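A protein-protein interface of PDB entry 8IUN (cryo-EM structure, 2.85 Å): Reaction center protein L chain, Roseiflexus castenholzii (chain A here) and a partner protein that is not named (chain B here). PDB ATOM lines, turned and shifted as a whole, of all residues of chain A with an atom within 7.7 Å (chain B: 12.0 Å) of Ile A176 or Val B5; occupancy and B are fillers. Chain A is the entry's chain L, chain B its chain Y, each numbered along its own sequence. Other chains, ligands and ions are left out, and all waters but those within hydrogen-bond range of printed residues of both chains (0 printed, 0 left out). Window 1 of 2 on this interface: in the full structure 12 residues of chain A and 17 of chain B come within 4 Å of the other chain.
OG1 of Thr A287 is in hydrogen-bond range of O of Phe A283 (3.0 Å).
Among the printed residues, merely in contact across the chains: Leu A173 with Met B9 (3.6 Å), Leu A173 with Phe B12 (3.9 Å), Leu A173 with Val B13 (3.6 Å), Ile A176 with Val B5 (3.8 Å), Ala A177 with Met B1 (3.8 Å), Ala A177 with Ala B6 (3.99 Å), Phe A283 with Ala B6 (3.7 Å), Phe A283 with Met B9 (3.6 Å) and Phe A283 with Leu B10 (3.6 Å).
Of chain B, only Val B5 (3.8 Å) comes within 4 Å of Ile A176. No residue of chain B comes within 4 Å of Trp A172. No residue of chain B comes within 4 Å of Pro A175. No residue of chain B comes within 4 Å of Gly A179. No residue of chain B comes within 4 Å of Ala A180. Of the printed residues of chain A, Phe B12 touches Leu A173 (3.9 Å). Of the printed residues of chain A, Met B1 touches Ala A177. The nearest residue of chain B that does not touch Ile A176 is Met B9 (4.1 Å). The nearest printed residue of chain A that does not touch Met B1 is Thr A287 (4.05 Å).
Printed residues of chain B that touch a printed residue of chain A: Met B1, Val B5, Ala B6, Met B9, Leu B10, Phe B12 and Val B13. Hydrophobic or aromatic side chains of chain B that line the printed part of chain A: Met B1, Val B5, Met B9, Leu B10, Phe B12 and Val B13. Of the 17 printed residues of chain A, 4 touch a printed residue of chain B. Hydrophobic or aromatic side chains of chain A that line the printed part of chain B: Leu A173, Ile A176, Ala A177 and Phe A283. Along chain A the printed residues that touch a printed residue of chain B span positions 173 to 283. Among the printed residues, no Asp or Glu carboxylate lies within 4 Å of a Lys or Arg side-chain nitrogen of the other chain.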
ATOM      1  N   LEU A 114     -22.703 -22.256   2.733  1.00  0.00           N
ATOM      2  CA  LEU A 114     -21.798 -22.560   3.834  1.00  0.00           C
ATOM      3  C   LEU A 114     -20.345 -22.267   3.489  1.00  0.00           C
ATOM      4  O   LEU A 114     -19.444 -22.936   4.008  1.00  0.00           O
ATOM      5  CB  LEU A 114     -21.956 -24.019   4.263  1.00  0.00           C
ATOM      6  CG  LEU A 114     -23.208 -24.452   5.034  1.00  0.00           C
ATOM      7  CD1 LEU A 114     -23.313 -25.955   5.041  1.00  0.00           C
ATOM      8  CD2 LEU A 114     -23.195 -23.930   6.453  1.00  0.00           C
ATOM      9  N   THR A 169     -26.335 -25.460  19.242  1.00  0.00           N
ATOM     10  CA  THR A 169     -27.528 -25.664  18.430  1.00  0.00           C
ATOM     11  C   THR A 169     -27.897 -24.403  17.663  1.00  0.00           C
ATOM     12  O   THR A 169     -28.233 -24.470  16.476  1.00  0.00           O
ATOM     13  CB  THR A 169     -28.698 -26.101  19.308  1.00  0.00           C
ATOM     14  OG1 THR A 169     -28.369 -27.321  19.979  1.00  0.00           O
ATOM     15  CG2 THR A 169     -29.941 -26.316  18.474  1.00  0.00           C
ATOM     16  N   LEU A 170     -27.842 -23.245  18.319  1.00  0.00           N
ATOM     17  CA  LEU A 170     -28.255 -22.017  17.648  1.00  0.00           C
ATOM     18  C   LEU A 170     -27.294 -21.627  16.530  1.00  0.00           C
ATOM     19  O   LEU A 170     -27.729 -21.149  15.479  1.00  0.00           O
ATOM     20  CB  LEU A 170     -28.392 -20.882  18.659  1.00  0.00           C
ATOM     21  CG  LEU A 170     -29.754 -20.725  19.331  1.00  0.00           C
ATOM     22  CD1 LEU A 170     -29.659 -19.780  20.504  1.00  0.00           C
ATOM     23  CD2 LEU A 170     -30.763 -20.212  18.341  1.00  0.00           C
ATOM     24  N   GLN A 171     -25.986 -21.813  16.730  1.00  0.00           N
ATOM     25  CA  GLN A 171     -25.011 -21.257  15.801  1.00  0.00           C
ATOM     26  C   GLN A 171     -24.337 -22.268  14.883  1.00  0.00           C
ATOM     27  O   GLN A 171     -23.747 -21.855  13.881  1.00  0.00           O
ATOM     28  CB  GLN A 171     -23.921 -20.489  16.565  1.00  0.00           C
ATOM     29  CG  GLN A 171     -24.406 -19.243  17.295  1.00  0.00           C
ATOM     30  CD  GLN A 171     -24.626 -18.051  16.385  1.00  0.00           C
ATOM     31  OE1 GLN A 171     -25.204 -18.172  15.315  1.00  0.00           O
ATOM     32  NE2 GLN A 171     -24.171 -16.890  16.815  1.00  0.00           N
ATOM     33  N   TRP A 172     -24.395 -23.566  15.184  1.00  0.00           N
ATOM     34  CA  TRP A 172     -23.730 -24.569  14.356  1.00  0.00           C
ATOM     35  C   TRP A 172     -24.703 -25.537  13.696  1.00  0.00           C
ATOM     36  O   TRP A 172     -24.706 -25.649  12.470  1.00  0.00           O
ATOM     37  CB  TRP A 172     -22.708 -25.352  15.188  1.00  0.00           C
ATOM     38  CG  TRP A 172     -21.473 -24.597  15.534  1.00  0.00           C
ATOM     39  CD1 TRP A 172     -21.250 -23.864  16.656  1.00  0.00           C
ATOM     40  CD2 TRP A 172     -20.279 -24.514  14.756  1.00  0.00           C
ATOM     41  NE1 TRP A 172     -19.996 -23.322  16.623  1.00  0.00           N
ATOM     42  CE2 TRP A 172     -19.377 -23.706  15.465  1.00  0.00           C
ATOM     43  CE3 TRP A 172     -19.887 -25.041  13.521  1.00  0.00           C
ATOM     44  CZ2 TRP A 172     -18.104 -23.413  14.987  1.00  0.00           C
ATOM     45  CZ3 TRP A 172     -18.627 -24.749  13.049  1.00  0.00           C
ATOM     46  CH2 TRP A 172     -17.749 -23.943  13.780  1.00  0.00           C
ATOM     47  N   LEU A 173     -25.526 -26.248  14.469  1.00  0.00           N
ATOM     48  CA  LEU A 173     -26.310 -27.347  13.913  1.00  0.00           C
ATOM     49  C   LEU A 173     -27.427 -26.837  13.016  1.00  0.00           C
ATOM     50  O   LEU A 173     -27.634 -27.349  11.909  1.00  0.00           O
ATOM     51  CB  LEU A 173     -26.883 -28.209  15.039  1.00  0.00           C
ATOM     52  CG  LEU A 173     -25.925 -28.756  16.097  1.00  0.00           C
ATOM     53  CD1 LEU A 173     -26.678 -29.579  17.108  1.00  0.00           C
ATOM     54  CD2 LEU A 173     -24.810 -29.571  15.478  1.00  0.00           C
ATOM     55  N   ARG A 174     -28.171 -25.839  13.487  1.00  0.00           N
ATOM     56  CA  ARG A 174     -29.303 -25.335  12.713  1.00  0.00           C
ATOM     57  C   ARG A 174     -28.876 -24.679  11.405  1.00  0.00           C
ATOM     58  O   ARG A 174     -29.481 -24.994  10.369  1.00  0.00           O
ATOM     59  CB  ARG A 174     -30.145 -24.402  13.590  1.00  0.00           C
ATOM     60  CG  ARG A 174     -31.522 -24.103  13.039  1.00  0.00           C
ATOM     61  CD  ARG A 174     -32.237 -23.076  13.886  1.00  0.00           C
ATOM     62  NE  ARG A 174     -33.466 -22.602  13.262  1.00  0.00           N
ATOM     63  CZ  ARG A 174     -33.559 -21.508  12.518  1.00  0.00           C
ATOM     64  NH1 ARG A 174     -32.506 -20.750  12.273  1.00  0.00           N
ATOM     65  NH2 ARG A 174     -34.737 -21.167  12.012  1.00  0.00           N
ATOM     66  N   PRO A 175     -27.879 -23.785  11.359  1.00  0.00           N
ATOM     67  CA  PRO A 175     -27.431 -23.273  10.053  1.00  0.00           C
ATOM     68  C   PRO A 175     -26.904 -24.337   9.101  1.00  0.00           C
ATOM     69  O   PRO A 175     -27.066 -24.191   7.886  1.00  0.00           O
ATOM     70  CB  PRO A 175     -26.336 -22.274  10.438  1.00  0.00           C
ATOM     71  CG  PRO A 175     -26.715 -21.822  11.760  1.00  0.00           C
ATOM     72  CD  PRO A 175     -27.254 -23.026  12.454  1.00  0.00           C
ATOM     73  N   ILE A 176     -26.253 -25.389   9.601  1.00  0.00           N
ATOM     74  CA  ILE A 176     -25.776 -26.451   8.720  1.00  0.00           C
ATOM     75  C   ILE A 176     -26.943 -27.249   8.158  1.00  0.00           C
ATOM     76  O   ILE A 176     -26.947 -27.620   6.979  1.00  0.00           O
ATOM     77  CB  ILE A 176     -24.771 -27.356   9.456  1.00  0.00           C
ATOM     78  CG1 ILE A 176     -23.473 -26.604   9.733  1.00  0.00           C
ATOM     79  CG2 ILE A 176     -24.462 -28.592   8.643  1.00  0.00           C
ATOM     80  CD1 ILE A 176     -22.458 -27.420  10.477  1.00  0.00           C
ATOM     81  N   ALA A 177     -27.952 -27.534   8.986  1.00  0.00           N
ATOM     82  CA  ALA A 177     -29.128 -28.246   8.491  1.00  0.00           C
ATOM     83  C   ALA A 177     -29.929 -27.394   7.511  1.00  0.00           C
ATOM     84  O   ALA A 177     -30.502 -27.921   6.552  1.00  0.00           O
ATOM     85  CB  ALA A 177     -30.000 -28.689   9.660  1.00  0.00           C
ATOM     86  N   MET A 178     -29.997 -26.080   7.744  1.00  0.00           N
ATOM     87  CA  MET A 178     -30.693 -25.184   6.826  1.00  0.00           C
ATOM     88  C   MET A 178     -29.909 -24.988   5.536  1.00  0.00           C
ATOM     89  O   MET A 178     -30.498 -24.875   4.457  1.00  0.00           O
ATOM     90  CB  MET A 178     -30.951 -23.836   7.497  1.00  0.00           C
ATOM     91  CG  MET A 178     -31.735 -23.892   8.798  1.00  0.00           C
ATOM     92  SD  MET A 178     -33.507 -23.972   8.608  1.00  0.00           S
ATOM     93  CE  MET A 178     -33.896 -22.274   8.272  1.00  0.00           C
ATOM     94  N   GLY A 179     -28.583 -24.917   5.625  1.00  0.00           N
ATOM     95  CA  GLY A 179     -27.749 -24.871   4.442  1.00  0.00           C
ATOM     96  C   GLY A 179     -26.969 -23.593   4.221  1.00  0.00           C
ATOM     97  O   GLY A 179     -26.389 -23.411   3.149  1.00  0.00           O
ATOM     98  N   ALA A 180     -26.936 -22.700   5.207  1.00  0.00           N
ATOM     99  CA  ALA A 180     -26.235 -21.434   5.050  1.00  0.00           C
ATOM    100  C   ALA A 180     -25.781 -20.918   6.406  1.00  0.00           C
ATOM    101  O   ALA A 180     -26.431 -21.156   7.424  1.00  0.00           O
ATOM    102  CB  ALA A 180     -27.117 -20.390   4.361  1.00  0.00           C
ATOM    103  N   TRP A 181     -24.647 -20.207   6.408  1.00  0.00           N
ATOM    104  CA  TRP A 181     -24.194 -19.501   7.603  1.00  0.00           C
ATOM    105  C   TRP A 181     -25.023 -18.261   7.894  1.00  0.00           C
ATOM    106  O   TRP A 181     -24.916 -17.710   8.991  1.00  0.00           O
ATOM    107  CB  TRP A 181     -22.723 -19.086   7.482  1.00  0.00           C
ATOM    108  CG  TRP A 181     -21.732 -20.207   7.544  1.00  0.00           C
ATOM    109  CD1 TRP A 181     -20.777 -20.497   6.625  1.00  0.00           C
ATOM    110  CD2 TRP A 181     -21.599 -21.184   8.584  1.00  0.00           C
ATOM    111  NE1 TRP A 181     -20.059 -21.595   7.017  1.00  0.00           N
ATOM    112  CE2 TRP A 181     -20.545 -22.037   8.217  1.00  0.00           C
ATOM    113  CE3 TRP A 181     -22.272 -21.422   9.786  1.00  0.00           C
ATOM    114  CZ2 TRP A 181     -20.146 -23.107   9.008  1.00  0.00           C
ATOM    115  CZ3 TRP A 181     -21.878 -22.482  10.565  1.00  0.00           C
ATOM    116  CH2 TRP A 181     -20.824 -23.312  10.177  1.00  0.00           C
ATOM    117  N   HIS A 183     -28.121 -18.110   8.443  1.00  0.00           N
ATOM    118  CA  HIS A 183     -29.216 -18.435   9.341  1.00  0.00           C
ATOM    119  C   HIS A 183     -28.839 -18.304  10.813  1.00  0.00           C
ATOM    120  O   HIS A 183     -29.679 -18.570  11.674  1.00  0.00           O
ATOM    121  CB  HIS A 183     -29.720 -19.857   9.061  1.00  0.00           C
ATOM    122  CG  HIS A 183     -30.412 -20.006   7.740  1.00  0.00           C
ATOM    123  ND1 HIS A 183     -31.637 -19.437   7.472  1.00  0.00           N
ATOM    124  CD2 HIS A 183     -30.054 -20.668   6.616  1.00  0.00           C
ATOM    125  CE1 HIS A 183     -32.000 -19.735   6.239  1.00  0.00           C
ATOM    126  NE2 HIS A 183     -31.058 -20.482   5.698  1.00  0.00           N
ATOM    127  N   PHE A 283     -34.645 -25.774  16.908  1.00  0.00           N
ATOM    128  CA  PHE A 283     -34.117 -26.584  15.815  1.00  0.00           C
ATOM    129  C   PHE A 283     -35.219 -26.996  14.848  1.00  0.00           C
ATOM    130  O   PHE A 283     -35.013 -26.990  13.630  1.00  0.00           O
ATOM    131  CB  PHE A 283     -33.392 -27.817  16.346  1.00  0.00           C
ATOM    132  CG  PHE A 283     -32.790 -28.668  15.261  1.00  0.00           C
ATOM    133  CD1 PHE A 283     -31.626 -28.277  14.627  1.00  0.00           C
ATOM    134  CD2 PHE A 283     -33.402 -29.841  14.860  1.00  0.00           C
ATOM    135  CE1 PHE A 283     -31.083 -29.039  13.626  1.00  0.00           C
ATOM    136  CE2 PHE A 283     -32.860 -30.605  13.857  1.00  0.00           C
ATOM    137  CZ  PHE A 283     -31.698 -30.201  13.240  1.00  0.00           C
ATOM    138  N   THR A 287     -36.593 -26.551  10.041  1.00  0.00           N
ATOM    139  CA  THR A 287     -36.610 -27.927   9.565  1.00  0.00           C
ATOM    140  C   THR A 287     -37.830 -28.635  10.135  1.00  0.00           C
ATOM    141  O   THR A 287     -38.127 -28.505  11.324  1.00  0.00           O
ATOM    142  CB  THR A 287     -35.337 -28.670   9.984  1.00  0.00           C
ATOM    143  OG1 THR A 287     -35.388 -28.945  11.387  1.00  0.00           O
ATOM    144  CG2 THR A 287     -34.107 -27.829   9.705  1.00  0.00           C
ATOM    145  N   MET B   1     -33.749 -28.811   1.271  1.00  0.00           N
ATOM    146  CA  MET B   1     -33.376 -29.542   2.476  1.00  0.00           C
ATOM    147  C   MET B   1     -32.693 -30.853   2.105  1.00  0.00           C
ATOM    148  O   MET B   1     -33.153 -31.575   1.223  1.00  0.00           O
ATOM    149  CB  MET B   1     -34.609 -29.803   3.345  1.00  0.00           C
ATOM    150  CG  MET B   1     -34.336 -30.578   4.627  1.00  0.00           C
ATOM    151  SD  MET B   1     -33.953 -29.521   6.030  1.00  0.00           S
ATOM    152  CE  MET B   1     -34.728 -27.993   5.527  1.00  0.00           C
ATOM    153  N   ASN B   2     -31.580 -31.151   2.779  1.00  0.00           N
ATOM    154  CA  ASN B   2     -30.846 -32.375   2.490  1.00  0.00           C
ATOM    155  C   ASN B   2     -31.553 -33.598   3.062  1.00  0.00           C
ATOM    156  O   ASN B   2     -31.597 -34.654   2.416  1.00  0.00           O
ATOM    157  CB  ASN B   2     -29.427 -32.263   3.039  1.00  0.00           C
ATOM    158  CG  ASN B   2     -28.462 -33.204   2.359  1.00  0.00           C
ATOM    159  OD1 ASN B   2     -28.800 -34.337   2.033  1.00  0.00           O
ATOM    160  ND2 ASN B   2     -27.245 -32.731   2.137  1.00  0.00           N
ATOM    161  N   TRP B   3     -32.087 -33.477   4.276  1.00  0.00           N
ATOM    162  CA  TRP B   3     -32.824 -34.508   5.006  1.00  0.00           C
ATOM    163  C   TRP B   3     -31.925 -35.609   5.544  1.00  0.00           C
ATOM    164  O   TRP B   3     -32.359 -36.401   6.381  1.00  0.00           O
ATOM    165  CB  TRP B   3     -33.920 -35.140   4.143  1.00  0.00           C
ATOM    166  CG  TRP B   3     -35.064 -34.239   3.852  1.00  0.00           C
ATOM    167  CD1 TRP B   3     -35.494 -33.841   2.627  1.00  0.00           C
ATOM    168  CD2 TRP B   3     -35.929 -33.616   4.805  1.00  0.00           C
ATOM    169  NE1 TRP B   3     -36.575 -33.009   2.753  1.00  0.00           N
ATOM    170  CE2 TRP B   3     -36.862 -32.853   4.082  1.00  0.00           C
ATOM    171  CE3 TRP B   3     -36.004 -33.627   6.200  1.00  0.00           C
ATOM    172  CZ2 TRP B   3     -37.857 -32.112   4.704  1.00  0.00           C
ATOM    173  CZ3 TRP B   3     -36.991 -32.889   6.812  1.00  0.00           C
ATOM    174  CH2 TRP B   3     -37.906 -32.143   6.068  1.00  0.00           C
ATOM    175  N   ILE B   4     -30.665 -35.642   5.135  1.00  0.00           N
ATOM    176  CA  ILE B   4     -29.687 -36.552   5.714  1.00  0.00           C
ATOM    177  C   ILE B   4     -28.779 -35.820   6.685  1.00  0.00           C
ATOM    178  O   ILE B   4     -28.435 -36.344   7.743  1.00  0.00           O
ATOM    179  CB  ILE B   4     -28.879 -37.259   4.605  1.00  0.00           C
ATOM    180  CG1 ILE B   4     -29.819 -37.931   3.609  1.00  0.00           C
ATOM    181  CG2 ILE B   4     -27.936 -38.289   5.202  1.00  0.00           C
ATOM    182  CD1 ILE B   4     -29.115 -38.806   2.614  1.00  0.00           C
ATOM    183  N   VAL B   5     -28.383 -34.596   6.336  1.00  0.00           N
ATOM    184  CA  VAL B   5     -27.668 -33.744   7.278  1.00  0.00           C
ATOM    185  C   VAL B   5     -28.592 -33.313   8.409  1.00  0.00           C
ATOM    186  O   VAL B   5     -28.190 -33.271   9.579  1.00  0.00           O
ATOM    187  CB  VAL B   5     -27.065 -32.535   6.541  1.00  0.00           C
ATOM    188  CG1 VAL B   5     -26.264 -31.676   7.493  1.00  0.00           C
ATOM    189  CG2 VAL B   5     -26.202 -33.005   5.390  1.00  0.00           C
ATOM    190  N   ALA B   6     -29.846 -32.994   8.082  1.00  0.00           N
ATOM    191  CA  ALA B   6     -30.795 -32.564   9.102  1.00  0.00           C
ATOM    192  C   ALA B   6     -31.034 -33.657  10.137  1.00  0.00           C
ATOM    193  O   ALA B   6     -31.206 -33.369  11.325  1.00  0.00           O
ATOM    194  CB  ALA B   6     -32.109 -32.141   8.448  1.00  0.00           C
ATOM    195  N   THR B   7     -31.028 -34.920   9.710  1.00  0.00           N
ATOM    196  CA  THR B   7     -31.238 -36.015  10.652  1.00  0.00           C
ATOM    197  C   THR B   7     -30.043 -36.196  11.583  1.00  0.00           C
ATOM    198  O   THR B   7     -30.218 -36.461  12.777  1.00  0.00           O
ATOM    199  CB  THR B   7     -31.539 -37.304   9.894  1.00  0.00           C
ATOM    200  OG1 THR B   7     -32.668 -37.095   9.040  1.00  0.00           O
ATOM    201  CG2 THR B   7     -31.862 -38.416  10.863  1.00  0.00           C
ATOM    202  N   PHE B   8     -28.821 -36.049  11.068  1.00  0.00           N
ATOM    203  CA  PHE B   8     -27.647 -36.111  11.936  1.00  0.00           C
ATOM    204  C   PHE B   8     -27.631 -34.957  12.934  1.00  0.00           C
ATOM    205  O   PHE B   8     -27.276 -35.143  14.106  1.00  0.00           O
ATOM    206  CB  PHE B   8     -26.367 -36.115  11.100  1.00  0.00           C
ATOM    207  CG  PHE B   8     -26.027 -37.456  10.513  1.00  0.00           C
ATOM    208  CD1 PHE B   8     -25.595 -38.491  11.320  1.00  0.00           C
ATOM    209  CD2 PHE B   8     -26.117 -37.675   9.151  1.00  0.00           C
ATOM    210  CE1 PHE B   8     -25.278 -39.722  10.782  1.00  0.00           C
ATOM    211  CE2 PHE B   8     -25.800 -38.906   8.610  1.00  0.00           C
ATOM    212  CZ  PHE B   8     -25.381 -39.927   9.425  1.00  0.00           C
ATOM    213  N   MET B   9     -28.007 -33.755  12.491  1.00  0.00           N
ATOM    214  CA  MET B   9     -28.081 -32.630  13.418  1.00  0.00           C
ATOM    215  C   MET B   9     -29.155 -32.855  14.476  1.00  0.00           C
ATOM    216  O   MET B   9     -28.967 -32.501  15.647  1.00  0.00           O
ATOM    217  CB  MET B   9     -28.337 -31.336  12.652  1.00  0.00           C
ATOM    218  CG  MET B   9     -27.314 -31.046  11.568  1.00  0.00           C
ATOM    219  SD  MET B   9     -25.671 -30.724  12.213  1.00  0.00           S
ATOM    220  CE  MET B   9     -24.692 -31.776  11.163  1.00  0.00           C
ATOM    221  N   LEU B  10     -30.286 -33.447  14.087  1.00  0.00           N
ATOM    222  CA  LEU B  10     -31.316 -33.792  15.059  1.00  0.00           C
ATOM    223  C   LEU B  10     -30.803 -34.810  16.067  1.00  0.00           C
ATOM    224  O   LEU B  10     -31.123 -34.733  17.258  1.00  0.00           O
ATOM    225  CB  LEU B  10     -32.552 -34.324  14.338  1.00  0.00           C
ATOM    226  CG  LEU B  10     -33.715 -34.877  15.161  1.00  0.00           C
ATOM    227  CD1 LEU B  10     -34.355 -33.803  16.018  1.00  0.00           C
ATOM    228  CD2 LEU B  10     -34.740 -35.507  14.245  1.00  0.00           C
ATOM    229  N   MET B  11     -30.007 -35.775  15.608  1.00  0.00           N
ATOM    230  CA  MET B  11     -29.439 -36.760  16.522  1.00  0.00           C
ATOM    231  C   MET B  11     -28.469 -36.117  17.504  1.00  0.00           C
ATOM    232  O   MET B  11     -28.390 -36.529  18.664  1.00  0.00           O
ATOM    233  CB  MET B  11     -28.755 -37.875  15.737  1.00  0.00           C
ATOM    234  CG  MET B  11     -29.723 -38.927  15.232  1.00  0.00           C
ATOM    235  SD  MET B  11     -31.114 -39.169  16.355  1.00  0.00           S
ATOM    236  CE  MET B  11     -32.470 -39.343  15.199  1.00  0.00           C
ATOM    237  N   PHE B  12     -27.707 -35.117  17.057  1.00  0.00           N
ATOM    238  CA  PHE B  12     -26.849 -34.379  17.987  1.00  0.00           C
ATOM    239  C   PHE B  12     -27.672 -33.605  19.013  1.00  0.00           C
ATOM    240  O   PHE B  12     -27.355 -33.606  20.213  1.00  0.00           O
ATOM    241  CB  PHE B  12     -25.929 -33.435  17.217  1.00  0.00           C
ATOM    242  CG  PHE B  12     -24.808 -34.131  16.511  1.00  0.00           C
ATOM    243  CD1 PHE B  12     -24.079 -35.115  17.151  1.00  0.00           C
ATOM    244  CD2 PHE B  12     -24.488 -33.813  15.206  1.00  0.00           C
ATOM    245  CE1 PHE B  12     -23.051 -35.761  16.506  1.00  0.00           C
ATOM    246  CE2 PHE B  12     -23.459 -34.459  14.553  1.00  0.00           C
ATOM    247  CZ  PHE B  12     -22.741 -35.434  15.204  1.00  0.00           C
ATOM    248  N   VAL B  13     -28.743 -32.951  18.562  1.00  0.00           N
ATOM    249  CA  VAL B  13     -29.626 -32.237  19.482  1.00  0.00           C
ATOM    250  C   VAL B  13     -30.200 -33.195  20.516  1.00  0.00           C
ATOM    251  O   VAL B  13     -30.342 -32.850  21.695  1.00  0.00           O
ATOM    252  CB  VAL B  13     -30.739 -31.507  18.704  1.00  0.00           C
ATOM    253  CG1 VAL B  13     -31.714 -30.851  19.652  1.00  0.00           C
ATOM    254  CG2 VAL B  13     -30.149 -30.475  17.771  1.00  0.00           C
ATOM    255  N   LEU B  14     -30.545 -34.412  20.096  1.00  0.00           N
ATOM    256  CA  LEU B  14     -31.105 -35.385  21.029  1.00  0.00           C
ATOM    257  C   LEU B  14     -30.050 -35.919  21.991  1.00  0.00           C
ATOM    258  O   LEU B  14     -30.315 -36.055  23.188  1.00  0.00           O
ATOM    259  CB  LEU B  14     -31.761 -36.532  20.266  1.00  0.00           C
ATOM    260  CG  LEU B  14     -33.046 -36.190  19.520  1.00  0.00           C
ATOM    261  CD1 LEU B  14     -33.638 -37.438  18.902  1.00  0.00           C
ATOM    262  CD2 LEU B  14     -34.039 -35.521  20.450  1.00  0.00           C
